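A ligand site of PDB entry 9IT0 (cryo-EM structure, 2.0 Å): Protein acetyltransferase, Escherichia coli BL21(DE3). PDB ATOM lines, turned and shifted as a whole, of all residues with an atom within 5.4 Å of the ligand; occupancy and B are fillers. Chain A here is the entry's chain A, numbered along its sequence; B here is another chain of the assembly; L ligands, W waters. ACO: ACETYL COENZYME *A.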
ATOM      1  N   ILE A  18      -3.725   4.255  27.180  1.00  0.00           N
ATOM      2  CA  ILE A  18      -3.590   3.389  26.016  1.00  0.00           C
ATOM      3  C   ILE A  18      -4.394   2.127  26.255  1.00  0.00           C
ATOM      4  O   ILE A  18      -4.165   1.414  27.241  1.00  0.00           O
ATOM      5  CB  ILE A  18      -2.115   3.066  25.734  1.00  0.00           C
ATOM      6  CG1 ILE A  18      -1.224   4.300  25.959  1.00  0.00           C
ATOM      7  CG2 ILE A  18      -1.938   2.521  24.321  1.00  0.00           C
ATOM      8  CD1 ILE A  18      -1.621   5.533  25.161  1.00  0.00           C
ATOM      9  N   GLY A  19      -5.329   1.832  25.361  1.00  0.00           N
ATOM     10  CA  GLY A  19      -6.186   0.667  25.487  1.00  0.00           C
ATOM     11  C   GLY A  19      -7.505   0.906  26.201  1.00  0.00           C
ATOM     12  O   GLY A  19      -8.145  -0.070  26.613  1.00  0.00           O
ATOM     13  N   ALA A  20      -7.937   2.156  26.353  1.00  0.00           N
ATOM     14  CA  ALA A  20      -9.249   2.439  26.918  1.00  0.00           C
ATOM     15  C   ALA A  20     -10.331   1.735  26.116  1.00  0.00           C
ATOM     16  O   ALA A  20     -10.245   1.637  24.882  1.00  0.00           O
ATOM     17  CB  ALA A  20      -9.497   3.943  26.949  1.00  0.00           C
ATOM     18  N   SER A  21     -11.362   1.245  26.808  1.00  0.00           N
ATOM     19  CA  SER A  21     -12.376   0.440  26.162  1.00  0.00           C
ATOM     20  C   SER A  21     -13.723   0.633  26.866  1.00  0.00           C
ATOM     21  O   SER A  21     -13.776   1.012  28.038  1.00  0.00           O
ATOM     22  CB  SER A  21     -12.004  -1.050  26.159  1.00  0.00           C
ATOM     23  OG  SER A  21     -13.152  -1.866  26.238  1.00  0.00           O
ATOM     24  N   MET A  22     -14.787   0.365  26.129  1.00  0.00           N
ATOM     25  CA  MET A  22     -16.156   0.496  26.637  1.00  0.00           C
ATOM     26  C   MET A  22     -16.699  -0.795  27.245  1.00  0.00           C
ATOM     27  O   MET A  22     -17.830  -0.780  27.755  1.00  0.00           O
ATOM     28  CB  MET A  22     -17.098   0.959  25.522  1.00  0.00           C
ATOM     29  CG  MET A  22     -17.276   2.465  25.434  1.00  0.00           C
ATOM     30  SD  MET A  22     -18.342   3.140  26.713  1.00  0.00           S
ATOM     31  CE  MET A  22     -19.809   3.564  25.772  1.00  0.00           C
ATOM     32  N   LYS A  23     -15.949  -1.888  27.202  1.00  0.00           N
ATOM     33  CA  LYS A  23     -16.454  -3.152  27.744  1.00  0.00           C
ATOM     34  C   LYS A  23     -16.310  -3.148  29.266  1.00  0.00           C
ATOM     35  O   LYS A  23     -15.210  -2.942  29.779  1.00  0.00           O
ATOM     36  CB  LYS A  23     -15.701  -4.330  27.145  1.00  0.00           C
ATOM     37  CG  LYS A  23     -16.233  -4.756  25.780  1.00  0.00           C
ATOM     38  CD  LYS A  23     -15.135  -5.007  24.754  1.00  0.00           C
ATOM     39  CE  LYS A  23     -14.804  -6.485  24.659  1.00  0.00           C
ATOM     40  NZ  LYS A  23     -14.075  -6.810  23.393  1.00  0.00           N
ATOM     41  N   ARG A  26     -13.200  -4.833  31.201  1.00  0.00           N
ATOM     42  CA  ARG A  26     -11.837  -4.594  30.742  1.00  0.00           C
ATOM     43  C   ARG A  26     -11.062  -3.735  31.737  1.00  0.00           C
ATOM     44  O   ARG A  26     -11.643  -2.987  32.540  1.00  0.00           O
ATOM     45  CB  ARG A  26     -11.849  -3.917  29.364  1.00  0.00           C
ATOM     46  CG  ARG A  26     -12.015  -4.869  28.189  1.00  0.00           C
ATOM     47  CD  ARG A  26     -10.893  -5.890  28.107  1.00  0.00           C
ATOM     48  NE  ARG A  26     -10.628  -6.304  26.736  1.00  0.00           N
ATOM     49  CZ  ARG A  26      -9.718  -7.217  26.395  1.00  0.00           C
ATOM     50  NH1 ARG A  26      -8.970  -7.825  27.304  1.00  0.00           N
ATOM     51  NH2 ARG A  26      -9.560  -7.512  25.109  1.00  0.00           N
ATOM     52  N   ALA A  27      -9.737  -3.857  31.684  1.00  0.00           N
ATOM     53  CA  ALA A  27      -8.881  -3.081  32.582  1.00  0.00           C
ATOM     54  C   ALA A  27      -8.882  -1.597  32.220  1.00  0.00           C
ATOM     55  O   ALA A  27      -8.896  -0.733  33.098  1.00  0.00           O
ATOM     56  CB  ALA A  27      -7.454  -3.640  32.543  1.00  0.00           C
ATOM     57  N   VAL A  47      -6.840   6.567  23.997  1.00  0.00           N
ATOM     58  CA  VAL A  47      -6.218   6.186  22.733  1.00  0.00           C
ATOM     59  C   VAL A  47      -6.602   4.746  22.430  1.00  0.00           C
ATOM     60  O   VAL A  47      -6.298   3.836  23.209  1.00  0.00           O
ATOM     61  CB  VAL A  47      -4.684   6.326  22.770  1.00  0.00           C
ATOM     62  CG1 VAL A  47      -4.049   5.784  21.496  1.00  0.00           C
ATOM     63  CG2 VAL A  47      -4.280   7.777  23.002  1.00  0.00           C
ATOM     64  N   THR A  48      -7.290   4.534  21.296  1.00  0.00           N
ATOM     65  CA  THR A  48      -7.721   3.191  20.897  1.00  0.00           C
ATOM     66  C   THR A  48      -8.235   3.184  19.457  1.00  0.00           C
ATOM     67  O   THR A  48      -8.828   4.179  19.012  1.00  0.00           O
ATOM     68  CB  THR A  48      -8.815   2.667  21.831  1.00  0.00           C
ATOM     69  OG1 THR A  48      -9.324   1.430  21.334  1.00  0.00           O
ATOM     70  CG2 THR A  48      -9.945   3.679  21.954  1.00  0.00           C
ATOM     71  N   PRO A  49      -8.040   2.105  18.703  1.00  0.00           N
ATOM     72  CA  PRO A  49      -8.574   2.015  17.340  1.00  0.00           C
ATOM     73  C   PRO A  49      -9.972   1.432  17.224  1.00  0.00           C
ATOM     74  O   PRO A  49     -10.473   1.310  16.099  1.00  0.00           O
ATOM     75  CB  PRO A  49      -7.551   1.102  16.648  1.00  0.00           C
ATOM     76  CG  PRO A  49      -7.153   0.146  17.730  1.00  0.00           C
ATOM     77  CD  PRO A  49      -7.254   0.903  19.040  1.00  0.00           C
ATOM     78  N   ALA A  50     -10.618   1.078  18.336  1.00  0.00           N
ATOM     79  CA  ALA A  50     -11.869   0.317  18.293  1.00  0.00           C
ATOM     80  C   ALA A  50     -13.077   1.105  18.781  1.00  0.00           C
ATOM     81  O   ALA A  50     -14.196   0.565  18.743  1.00  0.00           O
ATOM     82  CB  ALA A  50     -11.724  -0.956  19.127  1.00  0.00           C
ATOM     83  N   TRP A  51     -12.905   2.346  19.223  1.00  0.00           N
ATOM     84  CA  TRP A  51     -14.035   3.135  19.718  1.00  0.00           C
ATOM     85  C   TRP A  51     -13.839   4.604  19.340  1.00  0.00           C
ATOM     86  O   TRP A  51     -12.725   5.129  19.405  1.00  0.00           O
ATOM     87  CB  TRP A  51     -14.179   3.017  21.247  1.00  0.00           C
ATOM     88  CG  TRP A  51     -14.241   1.607  21.737  1.00  0.00           C
ATOM     89  CD1 TRP A  51     -13.219   0.878  22.277  1.00  0.00           C
ATOM     90  CD2 TRP A  51     -15.382   0.739  21.737  1.00  0.00           C
ATOM     91  NE1 TRP A  51     -13.651  -0.382  22.606  1.00  0.00           N
ATOM     92  CE2 TRP A  51     -14.979  -0.487  22.286  1.00  0.00           C
ATOM     93  CE3 TRP A  51     -16.713   0.883  21.321  1.00  0.00           C
ATOM     94  CZ2 TRP A  51     -15.854  -1.568  22.436  1.00  0.00           C
ATOM     95  CZ3 TRP A  51     -17.579  -0.178  21.472  1.00  0.00           C
ATOM     96  CH2 TRP A  51     -17.150  -1.391  22.028  1.00  0.00           C
ATOM     97  N   CYS A  76      -2.506  -0.496  28.981  1.00  0.00           N
ATOM     98  CA  CYS A  76      -3.524  -1.462  29.389  1.00  0.00           C
ATOM     99  C   CYS A  76      -3.684  -2.570  28.350  1.00  0.00           C
ATOM    100  O   CYS A  76      -4.788  -3.057  28.123  1.00  0.00           O
ATOM    101  CB  CYS A  76      -4.863  -0.766  29.631  1.00  0.00           C
ATOM    102  SG  CYS A  76      -4.785   0.633  30.767  1.00  0.00           S
ATOM    103  N   THR A  77      -2.588  -3.001  27.723  1.00  0.00           N
ATOM    104  CA  THR A  77      -2.624  -3.878  26.568  1.00  0.00           C
ATOM    105  C   THR A  77      -1.771  -5.123  26.803  1.00  0.00           C
ATOM    106  O   THR A  77      -1.063  -5.247  27.800  1.00  0.00           O
ATOM    107  CB  THR A  77      -2.136  -3.143  25.314  1.00  0.00           C
ATOM    108  OG1 THR A  77      -0.978  -2.347  25.635  1.00  0.00           O
ATOM    109  CG2 THR A  77      -3.223  -2.229  24.762  1.00  0.00           C
ATOM    110  N   ASN A  78      -1.848  -6.051  25.846  1.00  0.00           N
ATOM    111  CA  ASN A  78      -1.103  -7.305  25.931  1.00  0.00           C
ATOM    112  C   ASN A  78       0.400  -7.047  25.913  1.00  0.00           C
ATOM    113  O   ASN A  78       0.888  -6.111  25.277  1.00  0.00           O
ATOM    114  CB  ASN A  78      -1.482  -8.226  24.770  1.00  0.00           C
ATOM    115  CG  ASN A  78      -1.061  -9.666  24.998  1.00  0.00           C
ATOM    116  OD1 ASN A  78      -0.064 -10.132  24.436  1.00  0.00           O
ATOM    117  ND2 ASN A  78      -1.825 -10.396  25.804  1.00  0.00           N
ATOM    118  N   ARG A  81       2.788  -6.115  22.733  1.00  0.00           N
ATOM    119  CA  ARG A  81       2.851  -4.809  22.091  1.00  0.00           C
ATOM    120  C   ARG A  81       3.739  -3.825  22.847  1.00  0.00           C
ATOM    121  O   ARG A  81       3.850  -2.654  22.435  1.00  0.00           O
ATOM    122  CB  ARG A  81       1.437  -4.217  21.956  1.00  0.00           C
ATOM    123  CG  ARG A  81       0.354  -5.240  21.658  1.00  0.00           C
ATOM    124  CD  ARG A  81      -1.011  -4.582  21.443  1.00  0.00           C
ATOM    125  NE  ARG A  81      -2.085  -5.555  21.329  1.00  0.00           N
ATOM    126  CZ  ARG A  81      -2.541  -6.044  20.177  1.00  0.00           C
ATOM    127  NH1 ARG A  81      -2.027  -5.690  19.015  1.00  0.00           N
ATOM    128  NH2 ARG A  81      -3.552  -6.911  20.203  1.00  0.00           N
ATOM    129  N   LEU A  85       4.877   0.005  21.487  1.00  0.00           N
ATOM    130  CA  LEU A  85       4.164   1.132  22.075  1.00  0.00           C
ATOM    131  C   LEU A  85       5.126   2.051  22.835  1.00  0.00           C
ATOM    132  O   LEU A  85       4.998   3.275  22.771  1.00  0.00           O
ATOM    133  CB  LEU A  85       3.051   0.631  22.996  1.00  0.00           C
ATOM    134  CG  LEU A  85       1.878  -0.059  22.294  1.00  0.00           C
ATOM    135  CD1 LEU A  85       0.892  -0.639  23.305  1.00  0.00           C
ATOM    136  CD2 LEU A  85       1.172   0.889  21.339  1.00  0.00           C
ATOM    137  N   LEU A 100       1.242  -2.592  32.842  1.00  0.00           N
ATOM    138  CA  LEU A 100       0.356  -3.540  33.503  1.00  0.00           C
ATOM    139  C   LEU A 100       0.878  -4.968  33.513  1.00  0.00           C
ATOM    140  O   LEU A 100       0.712  -5.676  34.510  1.00  0.00           O
ATOM    141  CB  LEU A 100      -1.025  -3.493  32.836  1.00  0.00           C
ATOM    142  CG  LEU A 100      -2.060  -4.564  33.230  1.00  0.00           C
ATOM    143  CD1 LEU A 100      -2.468  -4.419  34.690  1.00  0.00           C
ATOM    144  CD2 LEU A 100      -3.281  -4.478  32.315  1.00  0.00           C
ATOM    145  N   SER A 101       1.507  -5.420  32.419  1.00  0.00           N
ATOM    146  CA  SER A 101       1.853  -6.829  32.276  1.00  0.00           C
ATOM    147  C   SER A 101       3.138  -6.981  31.480  1.00  0.00           C
ATOM    148  O   SER A 101       3.354  -6.281  30.496  1.00  0.00           O
ATOM    149  CB  SER A 101       0.716  -7.599  31.598  1.00  0.00           C
ATOM    150  OG  SER A 101       1.098  -8.932  31.299  1.00  0.00           O
ATOM    151  N   ASN A 125       3.655  -5.058  36.101  1.00  0.00           N
ATOM    152  CA  ASN A 125       2.739  -5.758  37.004  1.00  0.00           C
ATOM    153  C   ASN A 125       2.457  -4.922  38.244  1.00  0.00           C
ATOM    154  O   ASN A 125       2.340  -5.446  39.354  1.00  0.00           O
ATOM    155  CB  ASN A 125       3.292  -7.137  37.381  1.00  0.00           C
ATOM    156  CG  ASN A 125       3.828  -7.908  36.189  1.00  0.00           C
ATOM    157  OD1 ASN A 125       3.117  -8.134  35.219  1.00  0.00           O
ATOM    158  ND2 ASN A 125       5.098  -8.305  36.261  1.00  0.00           N
ATOM    159  N   SER A 126       2.337  -3.615  38.047  1.00  0.00           N
ATOM    160  CA  SER A 126       2.054  -2.682  39.130  1.00  0.00           C
ATOM    161  C   SER A 126       0.562  -2.404  39.225  1.00  0.00           C
ATOM    162  O   SER A 126      -0.139  -2.331  38.211  1.00  0.00           O
ATOM    163  CB  SER A 126       2.807  -1.371  38.931  1.00  0.00           C
ATOM    164  OG  SER A 126       2.254  -0.333  39.721  1.00  0.00           O
ATOM    165  N   LEU A 127       0.065  -2.260  40.465  1.00  0.00           N
ATOM    166  CA  LEU A 127      -1.352  -1.937  40.658  1.00  0.00           C
ATOM    167  C   LEU A 127      -1.649  -0.475  40.314  1.00  0.00           C
ATOM    168  O   LEU A 127      -2.779  -0.164  39.932  1.00  0.00           O
ATOM    169  CB  LEU A 127      -1.769  -2.245  42.100  1.00  0.00           C
ATOM    170  CG  LEU A 127      -3.218  -1.942  42.474  1.00  0.00           C
ATOM    171  CD1 LEU A 127      -4.176  -2.806  41.677  1.00  0.00           C
ATOM    172  CD2 LEU A 127      -3.445  -2.139  43.972  1.00  0.00           C
ATOM    173  N   PHE A 140      -5.786   0.372  39.200  1.00  0.00           N
ATOM    174  CA  PHE A 140      -6.755  -0.670  38.886  1.00  0.00           C
ATOM    175  C   PHE A 140      -7.430  -1.224  40.144  1.00  0.00           C
ATOM    176  O   PHE A 140      -7.915  -2.354  40.129  1.00  0.00           O
ATOM    177  CB  PHE A 140      -6.085  -1.817  38.118  1.00  0.00           C
ATOM    178  CG  PHE A 140      -5.393  -1.383  36.858  1.00  0.00           C
ATOM    179  CD1 PHE A 140      -6.096  -1.259  35.668  1.00  0.00           C
ATOM    180  CD2 PHE A 140      -4.034  -1.098  36.855  1.00  0.00           C
ATOM    181  CE1 PHE A 140      -5.451  -0.869  34.510  1.00  0.00           C
ATOM    182  CE2 PHE A 140      -3.389  -0.707  35.697  1.00  0.00           C
ATOM    183  CZ  PHE A 140      -4.102  -0.590  34.523  1.00  0.00           C
ATOM    184  N   ALA A 157      -0.050  -6.315  45.668  1.00  0.00           N
ATOM    185  CA  ALA A 157      -1.359  -5.739  45.366  1.00  0.00           C
ATOM    186  C   ALA A 157      -2.415  -6.148  46.393  1.00  0.00           C
ATOM    187  O   ALA A 157      -3.243  -5.328  46.805  1.00  0.00           O
ATOM    188  CB  ALA A 157      -1.794  -6.141  43.957  1.00  0.00           C
ATOM    189  N   ASP B 344      -4.315 -12.855  41.048  1.00  0.00           N
ATOM    190  CA  ASP B 344      -5.221 -11.764  41.403  1.00  0.00           C
ATOM    191  C   ASP B 344      -6.480 -11.755  40.558  1.00  0.00           C
ATOM    192  O   ASP B 344      -7.533 -11.285  41.029  1.00  0.00           O
ATOM    193  CB  ASP B 344      -4.506 -10.418  41.282  1.00  0.00           C
ATOM    194  CG  ASP B 344      -3.212 -10.357  42.089  1.00  0.00           C
ATOM    195  OD1 ASP B 344      -3.245 -10.694  43.287  1.00  0.00           O
ATOM    196  OD2 ASP B 344      -2.171  -9.971  41.520  1.00  0.00           O
ATOM    197  N   ASP B 345      -6.423 -12.253  39.328  1.00  0.00           N
ATOM    198  CA  ASP B 345      -7.546 -12.195  38.397  1.00  0.00           C
ATOM    199  C   ASP B 345      -8.363 -13.476  38.377  1.00  0.00           C
ATOM    200  O   ASP B 345      -9.021 -13.766  37.374  1.00  0.00           O
ATOM    201  CB  ASP B 345      -7.041 -11.867  36.988  1.00  0.00           C
ATOM    202  CG  ASP B 345      -6.289 -13.018  36.363  1.00  0.00           C
ATOM    203  OD1 ASP B 345      -5.678 -13.818  37.105  1.00  0.00           O
ATOM    204  OD2 ASP B 345      -6.305 -13.121  35.117  1.00  0.00           O
HETATM  205  N1A ACO L   1      -3.376   0.662  20.801  1.00  0.00           N
HETATM  206  C2A ACO L   1      -4.350   0.775  21.708  1.00  0.00           C
HETATM  207  N3A ACO L   1      -5.272  -0.128  22.063  1.00  0.00           N
HETATM  208  C4A ACO L   1      -5.127  -1.257  21.382  1.00  0.00           C
HETATM  209  C5A ACO L   1      -4.166  -1.530  20.415  1.00  0.00           C
HETATM  210  C6A ACO L   1      -3.255  -0.495  20.120  1.00  0.00           C
HETATM  211  N6A ACO L   1      -2.279  -0.599  19.217  1.00  0.00           N
HETATM  212  N7A ACO L   1      -4.315  -2.817  19.918  1.00  0.00           N
HETATM  213  C8A ACO L   1      -5.338  -3.284  20.587  1.00  0.00           C
HETATM  214  N9A ACO L   1      -5.888  -2.408  21.484  1.00  0.00           N
HETATM  215  C1B ACO L   1      -7.019  -2.642  22.368  1.00  0.00           C
HETATM  216  C2B ACO L   1      -7.828  -3.851  21.931  1.00  0.00           C
HETATM  217  O2B ACO L   1      -8.889  -3.302  21.162  1.00  0.00           O
HETATM  218  C3B ACO L   1      -8.471  -4.243  23.261  1.00  0.00           C
HETATM  219  O3B ACO L   1      -9.605  -3.359  23.366  1.00  0.00           O
HETATM  220  P3B ACO L   1     -11.077  -3.902  23.188  1.00  0.00           P
HETATM  221  O7A ACO L   1     -12.012  -2.865  23.675  1.00  0.00           O
HETATM  222  O8A ACO L   1     -11.176  -5.210  23.979  1.00  0.00           O
HETATM  223  O9A ACO L   1     -11.271  -4.242  21.709  1.00  0.00           O
HETATM  224  C4B ACO L   1      -7.457  -3.810  24.317  1.00  0.00           C
HETATM  225  O4B ACO L   1      -6.475  -3.031  23.605  1.00  0.00           O
HETATM  226  C5B ACO L   1      -6.733  -5.012  24.874  1.00  0.00           C
HETATM  227  O5B ACO L   1      -6.360  -5.881  23.782  1.00  0.00           O
HETATM  228  P1A ACO L   1      -5.078  -6.804  23.879  1.00  0.00           P
HETATM  229  O1A ACO L   1      -3.845  -5.986  23.911  1.00  0.00           O
HETATM  230  O2A ACO L   1      -5.132  -7.830  22.750  1.00  0.00           O
HETATM  231  O3A ACO L   1      -5.301  -7.580  25.243  1.00  0.00           O
HETATM  232  P2A ACO L   1      -5.708  -9.054  25.681  1.00  0.00           P
HETATM  233  O4A ACO L   1      -6.988  -9.468  25.093  1.00  0.00           O
HETATM  234  O5A ACO L   1      -4.528  -9.971  25.358  1.00  0.00           O
HETATM  235  O6A ACO L   1      -5.839  -8.937  27.264  1.00  0.00           O
HETATM  236  CBP ACO L   1      -4.695  -8.181  29.256  1.00  0.00           C
HETATM  237  CCP ACO L   1      -4.545  -8.615  27.800  1.00  0.00           C
HETATM  238  CDP ACO L   1      -5.365  -6.794  29.280  1.00  0.00           C
HETATM  239  CEP ACO L   1      -3.295  -8.068  29.876  1.00  0.00           C
HETATM  240  CAP ACO L   1      -5.550  -9.185  30.071  1.00  0.00           C
HETATM  241  OAP ACO L   1      -4.802 -10.386  30.057  1.00  0.00           O
HETATM  242  C9P ACO L   1      -5.765  -8.752  31.514  1.00  0.00           C
HETATM  243  O9P ACO L   1      -6.517  -7.819  31.770  1.00  0.00           O
HETATM  244  N8P ACO L   1      -5.113  -9.438  32.459  1.00  0.00           N
HETATM  245  C7P ACO L   1      -5.229  -9.119  33.876  1.00  0.00           C
HETATM  246  C6P ACO L   1      -4.083  -8.249  34.343  1.00  0.00           C
HETATM  247  C5P ACO L   1      -3.468  -8.743  35.636  1.00  0.00           C
HETATM  248  O5P ACO L   1      -2.453  -9.426  35.619  1.00  0.00           O
HETATM  249  N4P ACO L   1      -4.079  -8.399  36.771  1.00  0.00           N
HETATM  250  C3P ACO L   1      -5.284  -7.591  36.854  1.00  0.00           C
HETATM  251  C2P ACO L   1      -5.396  -6.900  38.204  1.00  0.00           C
HETATM  252  S1P ACO L   1      -4.250  -5.485  38.221  1.00  0.00           S
HETATM  253  C   ACO L   1      -3.097  -5.987  39.464  1.00  0.00           C
HETATM  254  O   ACO L   1      -3.409  -6.631  40.428  1.00  0.00           O
HETATM  255  CH3 ACO L   1      -1.700  -5.523  39.177  1.00  0.00           C
HETATM  256  O   HOH W   1      -0.261  -3.294  18.404  1.00  0.00           O
HETATM  257  O   HOH W   2      -8.658  -6.781  30.245  1.00  0.00           O
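The backbone NH of Asn 78 sits at hydrogen-bond distance from an oxygen (O1A) of the ligand, at 2.8 Å.
ND2 of Asn 78 sits at hydrogen-bond distance from O5A of the ligand (2.8 Å).
An oxygen (O7A) of the ligand is in hydrogen-bond range of the side-chain hydroxyl (OG) of Ser 21.
The guanidinium group (NE) of Arg 26 is in salt-bridge range of an oxygen (O8A) of the ligand.
An oxygen (O2A) of the ligand is in salt-bridge range of the guanidinium group (NH2) of Arg 81 (3.1 Å).
O7A of the ligand sits at hydrogen-bond distance from NE1 of Trp 51 (3.2 Å).
NZ of Lys 23 lies within salt-bridge range of O8A of the ligand (3.4 Å).
Ile 18 touches the ligand (CG2 to C2A, 3.96 Å).
Gly 19 touches the ligand.
O of Val 47 touches C2A of the ligand (3.9 Å).
Pro 49 touches the ligand.
O of Cys 76 touches CDP of the ligand (3.95 Å).
CG2 of Thr 77 touches O4B of the ligand, at 3.5 Å.
Ser 126 touches the ligand.
CA of Leu 127 touches CH3 of the ligand (3.9 Å).
CB of Ala 157 touches O of the ligand, 3.9 Å away.
OD2 of Asp 344 of chain B touches O of the ligand, at 3.7 Å.
Hydrophobic or aromatic side chains that line the ligand: Ile 18, Pro 49 and Ala 157.
Of the 27 residues printed, 16 come within 4 Å of the ligand.
The nearest printed residue that does not touch the ligand is Asn 125 (4.04 Å).
Water W2 lies within hydrogen-bond range of O9P of the ligand (2.8 Å), NH1 of Arg 26 (3.1 Å) and N of Ala 27 (3.4 Å).
Water W1 lies within hydrogen-bond range of NH1 of Arg 81 (3.0 Å) and N6A of the ligand (3.5 Å).
The side-chain hydroxyl (OG) of Ser 21 is in hydrogen-bond range of the backbone NH (N) of Lys 23 (3.0 Å).
The backbone NH of Gly 19 lies within hydrogen-bond range of the backbone carbonyl oxygen of Val 47.
The backbone carbonyl oxygen of Leu 127 is in hydrogen-bond range of the backbone NH of Phe 140 (3.1 Å).
The backbone NH (N) of Cys 76 is in hydrogen-bond range of the backbone carbonyl oxygen (O) of Ile 18 (3.1 Å).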
